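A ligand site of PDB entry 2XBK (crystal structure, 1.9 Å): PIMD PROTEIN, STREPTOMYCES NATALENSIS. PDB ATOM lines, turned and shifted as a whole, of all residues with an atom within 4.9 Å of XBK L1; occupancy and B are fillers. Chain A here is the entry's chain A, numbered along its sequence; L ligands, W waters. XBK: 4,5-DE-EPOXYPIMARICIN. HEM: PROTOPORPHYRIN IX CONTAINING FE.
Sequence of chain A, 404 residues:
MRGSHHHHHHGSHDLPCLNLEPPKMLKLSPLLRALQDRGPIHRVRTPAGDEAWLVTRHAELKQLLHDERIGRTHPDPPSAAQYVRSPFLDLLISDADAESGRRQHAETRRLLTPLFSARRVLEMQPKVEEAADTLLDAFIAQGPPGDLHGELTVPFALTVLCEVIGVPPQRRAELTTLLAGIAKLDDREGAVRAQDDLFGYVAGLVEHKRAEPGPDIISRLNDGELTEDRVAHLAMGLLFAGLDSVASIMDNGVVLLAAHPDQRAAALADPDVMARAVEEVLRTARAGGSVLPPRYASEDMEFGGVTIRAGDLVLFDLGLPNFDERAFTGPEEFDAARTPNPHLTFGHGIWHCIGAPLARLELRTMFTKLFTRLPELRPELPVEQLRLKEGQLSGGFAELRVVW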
ATOM      1  N   LEU A  20     -11.373  -0.176  29.663  1.00  0.00           N
ATOM      2  CA  LEU A  20     -11.208   1.260  29.479  1.00  0.00           C
ATOM      3  C   LEU A  20      -9.739   1.648  29.479  1.00  0.00           C
ATOM      4  O   LEU A  20      -9.392   2.789  29.830  1.00  0.00           O
ATOM      5  CB  LEU A  20     -12.002   2.024  30.530  1.00  0.00           C
ATOM      6  CG  LEU A  20     -13.509   1.679  30.554  1.00  0.00           C
ATOM      7  CD1 LEU A  20     -14.248   2.445  31.754  1.00  0.00           C
ATOM      8  CD2 LEU A  20     -14.170   2.049  29.253  1.00  0.00           C
ATOM      9  N   ARG A  72     -31.645   4.657  18.310  1.00  0.00           N
ATOM     10  CA  ARG A  72     -31.624   5.065  19.706  1.00  0.00           C
ATOM     11  C   ARG A  72     -32.979   4.833  20.372  1.00  0.00           C
ATOM     12  O   ARG A  72     -33.400   5.625  21.235  1.00  0.00           O
ATOM     13  CB  ARG A  72     -31.182   6.504  19.862  1.00  0.00           C
ATOM     14  CG  ARG A  72     -29.853   6.837  19.167  1.00  0.00           C
ATOM     15  CD  ARG A  72     -28.709   7.016  20.136  1.00  0.00           C
ATOM     16  NE  ARG A  72     -27.816   8.106  19.757  1.00  0.00           N
ATOM     17  CZ  ARG A  72     -26.587   7.973  19.292  1.00  0.00           C
ATOM     18  NH1 ARG A  72     -25.868   9.099  19.002  1.00  0.00           N
ATOM     19  NH2 ARG A  72     -26.049   6.748  19.125  1.00  0.00           N
ATOM     20  N   VAL A  84     -20.924   1.963  29.304  1.00  0.00           N
ATOM     21  CA  VAL A  84     -20.588   2.570  30.592  1.00  0.00           C
ATOM     22  C   VAL A  84     -21.923   3.126  31.122  1.00  0.00           C
ATOM     23  O   VAL A  84     -22.873   3.290  30.336  1.00  0.00           O
ATOM     24  CB  VAL A  84     -19.587   3.730  30.504  1.00  0.00           C
ATOM     25  CG1 VAL A  84     -18.113   3.225  30.151  1.00  0.00           C
ATOM     26  CG2 VAL A  84     -20.087   4.793  29.465  1.00  0.00           C
ATOM     27  N   PHE A  88     -26.154  11.058  31.516  1.00  0.00           N
ATOM     28  CA  PHE A  88     -26.201  11.841  30.265  1.00  0.00           C
ATOM     29  C   PHE A  88     -26.530  10.974  28.997  1.00  0.00           C
ATOM     30  O   PHE A  88     -27.396  11.344  28.174  1.00  0.00           O
ATOM     31  CB  PHE A  88     -24.942  12.710  30.069  1.00  0.00           C
ATOM     32  CG  PHE A  88     -25.050  13.739  28.973  1.00  0.00           C
ATOM     33  CD1 PHE A  88     -25.978  14.754  29.053  1.00  0.00           C
ATOM     34  CD2 PHE A  88     -24.277  13.645  27.814  1.00  0.00           C
ATOM     35  CE1 PHE A  88     -26.097  15.711  28.012  1.00  0.00           C
ATOM     36  CE2 PHE A  88     -24.392  14.611  26.805  1.00  0.00           C
ATOM     37  CZ  PHE A  88     -25.298  15.627  26.908  1.00  0.00           C
ATOM     38  N   LEU A  89     -25.869   9.838  28.820  1.00  0.00           N
ATOM     39  CA  LEU A  89     -26.178   9.017  27.672  1.00  0.00           C
ATOM     40  C   LEU A  89     -27.590   8.466  27.739  1.00  0.00           C
ATOM     41  O   LEU A  89     -28.254   8.390  26.698  1.00  0.00           O
ATOM     42  CB  LEU A  89     -25.168   7.867  27.485  1.00  0.00           C
ATOM     43  CG  LEU A  89     -23.696   8.326  27.138  1.00  0.00           C
ATOM     44  CD1 LEU A  89     -22.768   7.088  27.057  1.00  0.00           C
ATOM     45  CD2 LEU A  89     -23.527   9.189  25.906  1.00  0.00           C
ATOM     46  N   LEU A  92     -30.429   9.955  25.661  1.00  0.00           N
ATOM     47  CA  LEU A  92     -30.502   9.692  24.239  1.00  0.00           C
ATOM     48  C   LEU A  92     -31.450   8.585  23.819  1.00  0.00           C
ATOM     49  O   LEU A  92     -31.914   8.561  22.682  1.00  0.00           O
ATOM     50  CB  LEU A  92     -29.085   9.363  23.692  1.00  0.00           C
ATOM     51  CG  LEU A  92     -28.078  10.530  23.722  1.00  0.00           C
ATOM     52  CD1 LEU A  92     -26.723  10.029  23.198  1.00  0.00           C
ATOM     53  CD2 LEU A  92     -28.619  11.816  22.907  1.00  0.00           C
ATOM     54  N   LEU A 185     -18.803   9.265  35.327  1.00  0.00           N
ATOM     55  CA  LEU A 185     -19.291   7.897  35.215  1.00  0.00           C
ATOM     56  C   LEU A 185     -19.389   7.210  36.577  1.00  0.00           C
ATOM     57  O   LEU A 185     -20.070   6.209  36.716  1.00  0.00           O
ATOM     58  CB  LEU A 185     -18.368   7.055  34.303  1.00  0.00           C
ATOM     59  CG  LEU A 185     -18.255   7.608  32.889  1.00  0.00           C
ATOM     60  CD1 LEU A 185     -17.169   6.864  32.087  1.00  0.00           C
ATOM     61  CD2 LEU A 185     -19.655   7.551  32.156  1.00  0.00           C
ATOM     62  N   GLY A 237     -26.887  19.648  24.241  1.00  0.00           N
ATOM     63  CA  GLY A 237     -26.248  18.549  23.585  1.00  0.00           C
ATOM     64  C   GLY A 237     -25.096  19.035  22.708  1.00  0.00           C
ATOM     65  O   GLY A 237     -24.054  18.380  22.658  1.00  0.00           O
ATOM     66  N   LEU A 238     -25.325  20.141  21.974  1.00  0.00           N
ATOM     67  CA  LEU A 238     -24.289  20.759  21.201  1.00  0.00           C
ATOM     68  C   LEU A 238     -23.076  21.190  22.043  1.00  0.00           C
ATOM     69  O   LEU A 238     -21.961  20.981  21.627  1.00  0.00           O
ATOM     70  CB  LEU A 238     -24.828  21.991  20.403  1.00  0.00           C
ATOM     71  CG  LEU A 238     -25.747  21.710  19.224  1.00  0.00           C
ATOM     72  CD1 LEU A 238     -26.447  22.995  18.810  1.00  0.00           C
ATOM     73  CD2 LEU A 238     -24.931  21.273  18.126  1.00  0.00           C
ATOM     74  N   PHE A 240     -22.078  19.875  24.831  1.00  0.00           N
ATOM     75  CA  PHE A 240     -21.302  18.665  25.172  1.00  0.00           C
ATOM     76  C   PHE A 240     -20.627  18.036  23.944  1.00  0.00           C
ATOM     77  O   PHE A 240     -19.471  17.611  24.054  1.00  0.00           O
ATOM     78  CB  PHE A 240     -22.116  17.567  25.922  1.00  0.00           C
ATOM     79  CG  PHE A 240     -21.223  16.520  26.517  1.00  0.00           C
ATOM     80  CD1 PHE A 240     -20.511  16.792  27.685  1.00  0.00           C
ATOM     81  CD2 PHE A 240     -20.992  15.289  25.835  1.00  0.00           C
ATOM     82  CE1 PHE A 240     -19.580  15.881  28.211  1.00  0.00           C
ATOM     83  CE2 PHE A 240     -20.077  14.341  26.358  1.00  0.00           C
ATOM     84  CZ  PHE A 240     -19.361  14.625  27.544  1.00  0.00           C
ATOM     85  N   ALA A 241     -21.330  17.919  22.819  1.00  0.00           N
ATOM     86  CA  ALA A 241     -20.760  17.308  21.590  1.00  0.00           C
ATOM     87  C   ALA A 241     -19.547  18.009  20.997  1.00  0.00           C
ATOM     88  O   ALA A 241     -18.692  17.388  20.403  1.00  0.00           O
ATOM     89  CB  ALA A 241     -21.861  17.138  20.480  1.00  0.00           C
ATOM     90  N   ASP A 244     -15.173  18.426  24.322  1.00  0.00           N
ATOM     91  CA  ASP A 244     -14.033  17.500  24.534  1.00  0.00           C
ATOM     92  C   ASP A 244     -13.643  16.706  23.284  1.00  0.00           C
ATOM     93  O   ASP A 244     -12.584  16.170  23.234  1.00  0.00           O
ATOM     94  CB  ASP A 244     -14.404  16.480  25.589  1.00  0.00           C
ATOM     95  CG  ASP A 244     -14.528  17.097  26.911  1.00  0.00           C
ATOM     96  OD1 ASP A 244     -13.533  17.722  27.323  1.00  0.00           O
ATOM     97  OD2 ASP A 244     -15.643  16.981  27.520  1.00  0.00           O
ATOM     98  N   SER A 245     -14.530  16.604  22.322  1.00  0.00           N
ATOM     99  CA  SER A 245     -14.215  15.922  21.059  1.00  0.00           C
ATOM    100  C   SER A 245     -13.103  16.728  20.312  1.00  0.00           C
ATOM    101  O   SER A 245     -12.071  16.162  19.832  1.00  0.00           O
ATOM    102  CB  SER A 245     -15.488  15.930  20.186  1.00  0.00           C
ATOM    103  OG  SER A 245     -15.979  17.282  20.108  1.00  0.00           O
ATOM    104  N   SER A 248      -9.831  16.528  22.205  1.00  0.00           N
ATOM    105  CA  SER A 248      -9.148  15.259  22.071  1.00  0.00           C
ATOM    106  C   SER A 248      -8.413  15.182  20.733  1.00  0.00           C
ATOM    107  O   SER A 248      -7.209  14.810  20.647  1.00  0.00           O
ATOM    108  CB  SER A 248     -10.195  14.088  22.155  1.00  0.00           C
ATOM    109  OG  SER A 248      -9.577  12.856  21.693  1.00  0.00           O
ATOM    110  N   ILE A 249      -9.102  15.535  19.667  1.00  0.00           N
ATOM    111  CA  ILE A 249      -8.477  15.458  18.339  1.00  0.00           C
ATOM    112  C   ILE A 249      -7.287  16.486  18.307  1.00  0.00           C
ATOM    113  O   ILE A 249      -6.254  16.213  17.743  1.00  0.00           O
ATOM    114  CB  ILE A 249      -9.505  15.779  17.229  1.00  0.00           C
ATOM    115  CG1 ILE A 249     -10.680  14.769  17.294  1.00  0.00           C
ATOM    116  CG2 ILE A 249      -8.824  15.680  15.848  1.00  0.00           C
ATOM    117  CD1 ILE A 249     -10.281  13.217  17.214  1.00  0.00           C
ATOM    118  N   ARG A 286      -6.978   8.469  18.149  1.00  0.00           N
ATOM    119  CA  ARG A 286      -7.179   7.451  19.169  1.00  0.00           C
ATOM    120  C   ARG A 286      -7.348   6.093  18.477  1.00  0.00           C
ATOM    121  O   ARG A 286      -8.328   5.868  17.752  1.00  0.00           O
ATOM    122  CB  ARG A 286      -8.455   7.778  19.983  1.00  0.00           C
ATOM    123  CG  ARG A 286      -8.309   9.128  20.890  1.00  0.00           C
ATOM    124  CD  ARG A 286      -7.376   8.942  22.114  1.00  0.00           C
ATOM    125  NE  ARG A 286      -5.940   8.720  21.767  1.00  0.00           N
ATOM    126  CZ  ARG A 286      -4.996   8.420  22.689  1.00  0.00           C
ATOM    127  NH1 ARG A 286      -3.690   8.200  22.388  1.00  0.00           N
ATOM    128  NH2 ARG A 286      -5.384   8.337  23.954  1.00  0.00           N
ATOM    129  N   GLY A 288      -8.551   3.096  19.040  1.00  0.00           N
ATOM    130  CA  GLY A 288      -9.351   2.253  19.944  1.00  0.00           C
ATOM    131  C   GLY A 288      -9.859   3.036  21.150  1.00  0.00           C
ATOM    132  O   GLY A 288      -9.282   4.070  21.537  1.00  0.00           O
ATOM    133  N   GLY A 289     -10.979   2.584  21.725  1.00  0.00           N
ATOM    134  CA  GLY A 289     -11.556   3.266  22.897  1.00  0.00           C
ATOM    135  C   GLY A 289     -12.501   4.409  22.526  1.00  0.00           C
ATOM    136  O   GLY A 289     -13.134   5.023  23.412  1.00  0.00           O
ATOM    137  N   SER A 290     -12.609   4.719  21.235  1.00  0.00           N
ATOM    138  CA  SER A 290     -13.540   5.789  20.768  1.00  0.00           C
ATOM    139  C   SER A 290     -14.954   5.256  20.534  1.00  0.00           C
ATOM    140  O   SER A 290     -15.489   5.255  19.385  1.00  0.00           O
ATOM    141  CB  SER A 290     -12.998   6.489  19.522  1.00  0.00           C
ATOM    142  OG  SER A 290     -11.706   7.027  19.882  1.00  0.00           O
ATOM    143  N   VAL A 291     -15.559   4.833  21.631  1.00  0.00           N
ATOM    144  CA  VAL A 291     -16.848   4.149  21.563  1.00  0.00           C
ATOM    145  C   VAL A 291     -17.950   5.163  21.657  1.00  0.00           C
ATOM    146  O   VAL A 291     -17.995   5.938  22.641  1.00  0.00           O
ATOM    147  CB  VAL A 291     -16.943   3.093  22.688  1.00  0.00           C
ATOM    148  CG1 VAL A 291     -18.326   2.402  22.658  1.00  0.00           C
ATOM    149  CG2 VAL A 291     -15.778   2.079  22.517  1.00  0.00           C
ATOM    150  N   LEU A 292     -18.828   5.170  20.641  1.00  0.00           N
ATOM    151  CA  LEU A 292     -19.958   6.086  20.587  1.00  0.00           C
ATOM    152  C   LEU A 292     -21.118   5.757  21.567  1.00  0.00           C
ATOM    153  O   LEU A 292     -21.116   4.626  22.147  1.00  0.00           O
ATOM    154  CB  LEU A 292     -20.492   6.174  19.125  1.00  0.00           C
ATOM    155  CG  LEU A 292     -19.371   6.478  18.117  1.00  0.00           C
ATOM    156  CD1 LEU A 292     -19.945   6.559  16.658  1.00  0.00           C
ATOM    157  CD2 LEU A 292     -18.611   7.788  18.518  1.00  0.00           C
ATOM    158  N   PRO A 293     -22.119   6.717  21.761  1.00  0.00           N
ATOM    159  CA  PRO A 293     -23.316   6.453  22.521  1.00  0.00           C
ATOM    160  C   PRO A 293     -23.938   5.153  22.041  1.00  0.00           C
ATOM    161  O   PRO A 293     -23.798   4.770  20.854  1.00  0.00           O
ATOM    162  CB  PRO A 293     -24.236   7.636  22.182  1.00  0.00           C
ATOM    163  CG  PRO A 293     -23.281   8.789  22.003  1.00  0.00           C
ATOM    164  CD  PRO A 293     -22.020   8.145  21.413  1.00  0.00           C
ATOM    165  N   LEU A 388      -4.587   9.678  30.974  1.00  0.00           N
ATOM    166  CA  LEU A 388      -5.998   9.932  30.603  1.00  0.00           C
ATOM    167  C   LEU A 388      -6.868  10.152  31.845  1.00  0.00           C
ATOM    168  O   LEU A 388      -6.584   9.576  32.900  1.00  0.00           O
ATOM    169  CB  LEU A 388      -6.520   8.776  29.739  1.00  0.00           C
ATOM    170  CG  LEU A 388      -6.277   9.010  28.235  1.00  0.00           C
ATOM    171  CD1 LEU A 388      -4.808   9.234  27.942  1.00  0.00           C
ATOM    172  CD2 LEU A 388      -6.843   7.891  27.399  1.00  0.00           C
ATOM    173  N   GLN A 392     -14.806   9.519  33.419  1.00  0.00           N
ATOM    174  CA  GLN A 392     -15.438  10.638  32.743  1.00  0.00           C
ATOM    175  C   GLN A 392     -15.708  10.283  31.306  1.00  0.00           C
ATOM    176  O   GLN A 392     -14.799   9.889  30.577  1.00  0.00           O
ATOM    177  CB  GLN A 392     -14.564  11.888  32.793  1.00  0.00           C
ATOM    178  CG  GLN A 392     -15.308  13.153  32.438  1.00  0.00           C
ATOM    179  CD  GLN A 392     -14.508  14.386  32.800  1.00  0.00           C
ATOM    180  OE1 GLN A 392     -13.959  14.482  33.921  1.00  0.00           O
ATOM    181  NE2 GLN A 392     -14.388  15.322  31.860  1.00  0.00           N
ATOM    182  N   LEU A 393     -16.957  10.453  30.907  1.00  0.00           N
ATOM    183  CA  LEU A 393     -17.374  10.251  29.477  1.00  0.00           C
ATOM    184  C   LEU A 393     -16.667  11.287  28.607  1.00  0.00           C
ATOM    185  O   LEU A 393     -16.697  12.473  28.952  1.00  0.00           O
ATOM    186  CB  LEU A 393     -18.887  10.444  29.327  1.00  0.00           C
ATOM    187  CG  LEU A 393     -19.373  10.374  27.874  1.00  0.00           C
ATOM    188  CD1 LEU A 393     -19.289   8.950  27.301  1.00  0.00           C
ATOM    189  CD2 LEU A 393     -20.802  10.856  27.860  1.00  0.00           C
ATOM    190  N   SER A 394     -16.078  10.876  27.498  1.00  0.00           N
ATOM    191  CA  SER A 394     -15.332  11.806  26.662  1.00  0.00           C
ATOM    192  C   SER A 394     -14.203  12.542  27.396  1.00  0.00           C
ATOM    193  O   SER A 394     -13.857  13.651  27.042  1.00  0.00           O
ATOM    194  CB  SER A 394     -16.318  12.855  26.064  1.00  0.00           C
ATOM    195  OG  SER A 394     -15.887  13.235  24.797  1.00  0.00           O
ATOM    196  N   GLY A 395     -13.588  11.910  28.379  1.00  0.00           N
ATOM    197  CA  GLY A 395     -12.694  12.674  29.255  1.00  0.00           C
ATOM    198  C   GLY A 395     -11.345  13.154  28.697  1.00  0.00           C
ATOM    199  O   GLY A 395     -10.786  14.187  29.207  1.00  0.00           O
ATOM    200  N   GLY A 396     -10.783  12.448  27.714  1.00  0.00           N
ATOM    201  CA  GLY A 396      -9.528  12.880  27.134  1.00  0.00           C
ATOM    202  C   GLY A 396      -8.356  12.908  28.134  1.00  0.00           C
ATOM    203  O   GLY A 396      -8.374  12.173  29.140  1.00  0.00           O
HETATM  204  N   XBK L   1     -11.068   7.642  27.280  1.00  0.00           N
HETATM  205  C1  XBK L   1     -12.524  11.318  20.950  1.00  0.00           C
HETATM  206  O1  XBK L   1     -11.262  11.226  20.278  1.00  0.00           O
HETATM  207  C2  XBK L   1     -12.978   9.915  21.420  1.00  0.00           C
HETATM  208  O2  XBK L   1     -11.636   9.817  23.364  1.00  0.00           O
HETATM  209  C3  XBK L   1     -11.977   9.270  22.344  1.00  0.00           C
HETATM  210  O3  XBK L   1     -11.437   8.104  22.083  1.00  0.00           O
HETATM  211  C4  XBK L   1     -14.303  10.080  22.122  1.00  0.00           C
HETATM  212  O4  XBK L   1     -15.000   9.232  24.998  1.00  0.00           O
HETATM  213  C5  XBK L   1     -14.839   8.686  22.481  1.00  0.00           C
HETATM  214  O5  XBK L   1     -12.738   9.601  26.726  1.00  0.00           O
HETATM  215  C6  XBK L   1     -15.604   8.659  23.822  1.00  0.00           C
HETATM  216  O6  XBK L   1     -12.740   5.710  28.709  1.00  0.00           O
HETATM  217  C7  XBK L   1     -14.444   8.139  25.763  1.00  0.00           C
HETATM  218  O7  XBK L   1     -15.229   7.794  26.914  1.00  0.00           O
HETATM  219  C8  XBK L   1     -12.947   8.366  26.032  1.00  0.00           C
HETATM  220  O8  XBK L   1     -24.868  14.478  20.478  1.00  0.00           O
HETATM  221  C9  XBK L   1     -12.346   7.186  26.822  1.00  0.00           C
HETATM  222  O9  XBK L   1     -24.949  12.258  20.680  1.00  0.00           O
HETATM  223  C10 XBK L   1     -13.234   6.852  28.023  1.00  0.00           C
HETATM  224  O10 XBK L   1     -17.824  13.120  20.875  1.00  0.00           O
HETATM  225  C11 XBK L   1     -14.703   6.657  27.639  1.00  0.00           C
HETATM  226  O11 XBK L   1     -15.035  12.825  21.593  1.00  0.00           O
HETATM  227  C12 XBK L   1     -15.567   6.519  28.871  1.00  0.00           C
HETATM  228  O12 XBK L   1     -15.250  10.626  21.133  1.00  0.00           O
HETATM  229  C13 XBK L   1     -17.045   9.095  23.732  1.00  0.00           C
HETATM  230  C14 XBK L   1     -17.477  10.310  23.661  1.00  0.00           C
HETATM  231  C15 XBK L   1     -18.910  10.313  23.608  1.00  0.00           C
HETATM  232  C16 XBK L   1     -19.556  11.456  23.613  1.00  0.00           C
HETATM  233  C17 XBK L   1     -21.005  11.435  23.554  1.00  0.00           C
HETATM  234  C18 XBK L   1     -21.707  12.582  23.507  1.00  0.00           C
HETATM  235  C19 XBK L   1     -23.170  12.734  23.437  1.00  0.00           C
HETATM  236  C20 XBK L   1     -23.673  13.972  23.157  1.00  0.00           C
HETATM  237  C21 XBK L   1     -25.099  14.523  23.007  1.00  0.00           C
HETATM  238  C22 XBK L   1     -25.785  14.505  21.579  1.00  0.00           C
HETATM  239  C23 XBK L   1     -26.716  15.683  21.224  1.00  0.00           C
HETATM  240  C24 XBK L   1     -24.337  13.220  20.253  1.00  0.00           C
HETATM  241  C25 XBK L   1     -23.048  13.208  19.549  1.00  0.00           C
HETATM  242  C26 XBK L   1     -22.092  12.448  20.009  1.00  0.00           C
HETATM  243  C27 XBK L   1     -20.773  12.466  19.350  1.00  0.00           C
HETATM  244  C28 XBK L   1     -19.839  11.669  19.837  1.00  0.00           C
HETATM  245  C29 XBK L   1     -18.499  11.627  19.172  1.00  0.00           C
HETATM  246  C30 XBK L   1     -17.415  11.920  20.179  1.00  0.00           C
HETATM  247  C31 XBK L   1     -16.051  12.039  19.458  1.00  0.00           C
HETATM  248  C32 XBK L   1     -14.953  11.849  20.528  1.00  0.00           C
HETATM  249  C33 XBK L   1     -13.541  11.898  19.959  1.00  0.00           C
HETATM  250  CHA HEM L   2     -22.420  13.644  15.964  1.00  0.00           C
HETATM  251  CHB HEM L   2     -17.571  13.298  15.987  1.00  0.00           C
HETATM  252  CHC HEM L   2     -17.234  17.998  16.843  1.00  0.00           C
HETATM  253  CHD HEM L   2     -22.092  18.444  17.003  1.00  0.00           C
HETATM  254  C1A HEM L   2     -21.143  13.157  15.905  1.00  0.00           C
HETATM  255  C2A HEM L   2     -20.813  11.793  15.647  1.00  0.00           C
HETATM  256  C3A HEM L   2     -19.471  11.684  15.657  1.00  0.00           C
HETATM  257  C4A HEM L   2     -18.907  12.995  15.912  1.00  0.00           C
HETATM  258  CMA HEM L   2     -18.677  10.333  15.465  1.00  0.00           C
HETATM  259  CAA HEM L   2     -21.808  10.633  15.497  1.00  0.00           C
HETATM  260  CBA HEM L   2     -22.214  10.265  16.941  1.00  0.00           C
HETATM  261  CGA HEM L   2     -23.045   8.962  17.004  1.00  0.00           C
HETATM  262  O1A HEM L   2     -23.246   8.437  18.109  1.00  0.00           O
HETATM  263  O2A HEM L   2     -23.518   8.401  15.975  1.00  0.00           O
HETATM  264  C1B HEM L   2     -17.039  14.536  16.275  1.00  0.00           C
HETATM  265  C2B HEM L   2     -15.621  14.859  16.402  1.00  0.00           C
HETATM  266  C3B HEM L   2     -15.552  16.177  16.616  1.00  0.00           C
HETATM  267  C4B HEM L   2     -16.884  16.693  16.701  1.00  0.00           C
HETATM  268  CMB HEM L   2     -14.482  13.809  16.309  1.00  0.00           C
HETATM  269  CAB HEM L   2     -14.275  17.013  16.863  1.00  0.00           C
HETATM  270  CBB HEM L   2     -13.321  16.877  15.935  1.00  0.00           C
HETATM  271  C1C HEM L   2     -18.509  18.539  16.907  1.00  0.00           C
HETATM  272  C2C HEM L   2     -18.826  19.948  17.118  1.00  0.00           C
HETATM  273  C3C HEM L   2     -20.152  20.021  17.159  1.00  0.00           C
HETATM  274  C4C HEM L   2     -20.736  18.738  17.019  1.00  0.00           C
HETATM  275  CMC HEM L   2     -17.786  21.083  17.185  1.00  0.00           C
HETATM  276  CAC HEM L   2     -21.136  21.197  17.383  1.00  0.00           C
HETATM  277  CBC HEM L   2     -20.867  22.435  17.383  1.00  0.00           C
HETATM  278  C1D HEM L   2     -22.603  17.153  16.806  1.00  0.00           C
HETATM  279  C2D HEM L   2     -24.018  16.835  16.934  1.00  0.00           C
HETATM  280  C3D HEM L   2     -24.113  15.381  16.571  1.00  0.00           C
HETATM  281  C4D HEM L   2     -22.758  14.929  16.328  1.00  0.00           C
HETATM  282  CMD HEM L   2     -25.170  17.849  17.294  1.00  0.00           C
HETATM  283  CAD HEM L   2     -25.392  14.528  16.603  1.00  0.00           C
HETATM  284  CBD HEM L   2     -25.910  14.594  15.187  1.00  0.00           C
HETATM  285  CGD HEM L   2     -27.108  13.656  15.057  1.00  0.00           C
HETATM  286  O1D HEM L   2     -27.193  12.846  14.045  1.00  0.00           O
HETATM  287  O2D HEM L   2     -27.982  13.696  16.003  1.00  0.00           O
HETATM  288  NA  HEM L   2     -19.926  13.872  15.984  1.00  0.00           N
HETATM  289  NB  HEM L   2     -17.784  15.708  16.456  1.00  0.00           N
HETATM  290  NC  HEM L   2     -19.709  17.835  16.839  1.00  0.00           N
HETATM  291  ND  HEM L   2     -21.900  15.986  16.427  1.00  0.00           N
HETATM  292 FE   HEM L   2     -19.821  15.883  16.280  1.00  0.00          FE
HETATM  293  O   HOH W   1     -18.847  15.051  19.296  1.00  0.00           O
HETATM  294  O   HOH W   2      -9.829   6.517  23.345  1.00  0.00           O
HETATM  295  O   HOH W   3     -17.294  15.280  23.366  1.00  0.00           O
HETATM  296  O   HOH W   4     -10.310   9.754  29.566  1.00  0.00           O
HETATM  297  O   HOH W   5     -13.284  13.371  24.074  1.00  0.00           O
HETATM  298  O   HOH W   6     -11.767   3.855  27.049  1.00  0.00           O
HETATM  299  O   HOH W   7     -11.384   9.548  18.155  1.00  0.00           O
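The side-chain hydroxyl (OG) of Ser 245 sits at hydrogen-bond distance from the backbone carbonyl oxygen (O) of Ala 241. The guanidinium group (NH2) of Arg 72 is in hydrogen-bond range of the backbone carbonyl oxygen (O) of Pro 293.
CD2 of Leu 20 touches O6 of XBK L1 (3.97 Å). NH1 of Arg 72 touches O9 of XBK L1, 3.7 Å away. Phe 88 touches XBK L1 (CE2 to C20, 3.8 Å). Leu 92 touches XBK L1 (CD1 to O9, 3.8 Å). Leu 185 touches XBK L1. CA of Gly 237 touches C23 of XBK L1, at 3.7 Å. CD2 of Phe 240 touches C18 of XBK L1, 3.6 Å away. Ser 245 touches XBK L1 (CA to O11, 3.2 Å). CD1 of Ile 249 touches O1 of XBK L1, at 3.8 Å. Arg 286 touches XBK L1. Gly 289 touches XBK L1 (O to O3, 3.8 Å). O of Val 291 touches C13 of XBK L1 (3.5 Å). Leu 292 touches XBK L1 (CD2 to C29, 3.9 Å). Pro 293 touches XBK L1. Gln 392 touches XBK L1. Leu 393 touches XBK L1. Gly 396 touches XBK L1. Hydrophobic or aromatic side chains within 4 Å of XBK L1: Leu 20, Phe 88, Leu 92, Leu 185, Phe 240, Ile 249, Leu 292, Pro 293 and Leu 393. Within 4 Å of XBK L1: Leu 20, Arg 72, Phe 88, Leu 92, Leu 185, Gly 237, Phe 240, Ser 245, Ser 248, Ile 249, Arg 286, Gly 289, Ser 290, Val 291, Leu 292, Pro 293, Gln 392, Leu 393, Ser 394, Gly 395 and Gly 396. Along chain A the residues within 4 Å of XBK L1 span positions 20 to 396.
The side-chain hydroxyl (OG) of Ser 290 sits at hydrogen-bond distance from an oxygen (O3) of XBK L1, at 2.5 Å. OG of Ser 248 is in hydrogen-bond range of O1 of XBK L1. The backbone NH (N) of Gly 395 is in hydrogen-bond range of an oxygen (O5) of XBK L1, 3.0 Å away. O4 of XBK L1 lies close to N of Ser 394, 3.2 Å away. An oxygen (O11) of XBK L1 sits at hydrogen-bond distance from the side-chain hydroxyl (OG) of Ser 394, 3.3 Å away. O1A of HEM L2 lies within salt-bridge range of NH1 of Arg 72, at 2.8 Å.
Water W2 bridges an oxygen (O3) of XBK L1 and the backbone carbonyl oxygen of Gly 288. Water W1 lies within hydrogen-bond range of O of Ala 241 (2.6 Å) and O10 of XBK L1 (2.7 Å). Water W7 bridges O1 of XBK L1 (2.7 Å) and OG of Ser 290 (3.1 Å). Water W5 lies within hydrogen-bond range of OG of Ser 394, O of Asp 244 and O11 of XBK L1. Water W4 lies within hydrogen-bond range of O of Gly 396 and N of XBK L1. Water W3 lies within hydrogen-bond range of OG of Ser 394 (2.9 Å), N of Ser 245 (3.2 Å), O of Phe 240 (3.3 Å) and O10 of XBK L1 (3.3 Å).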
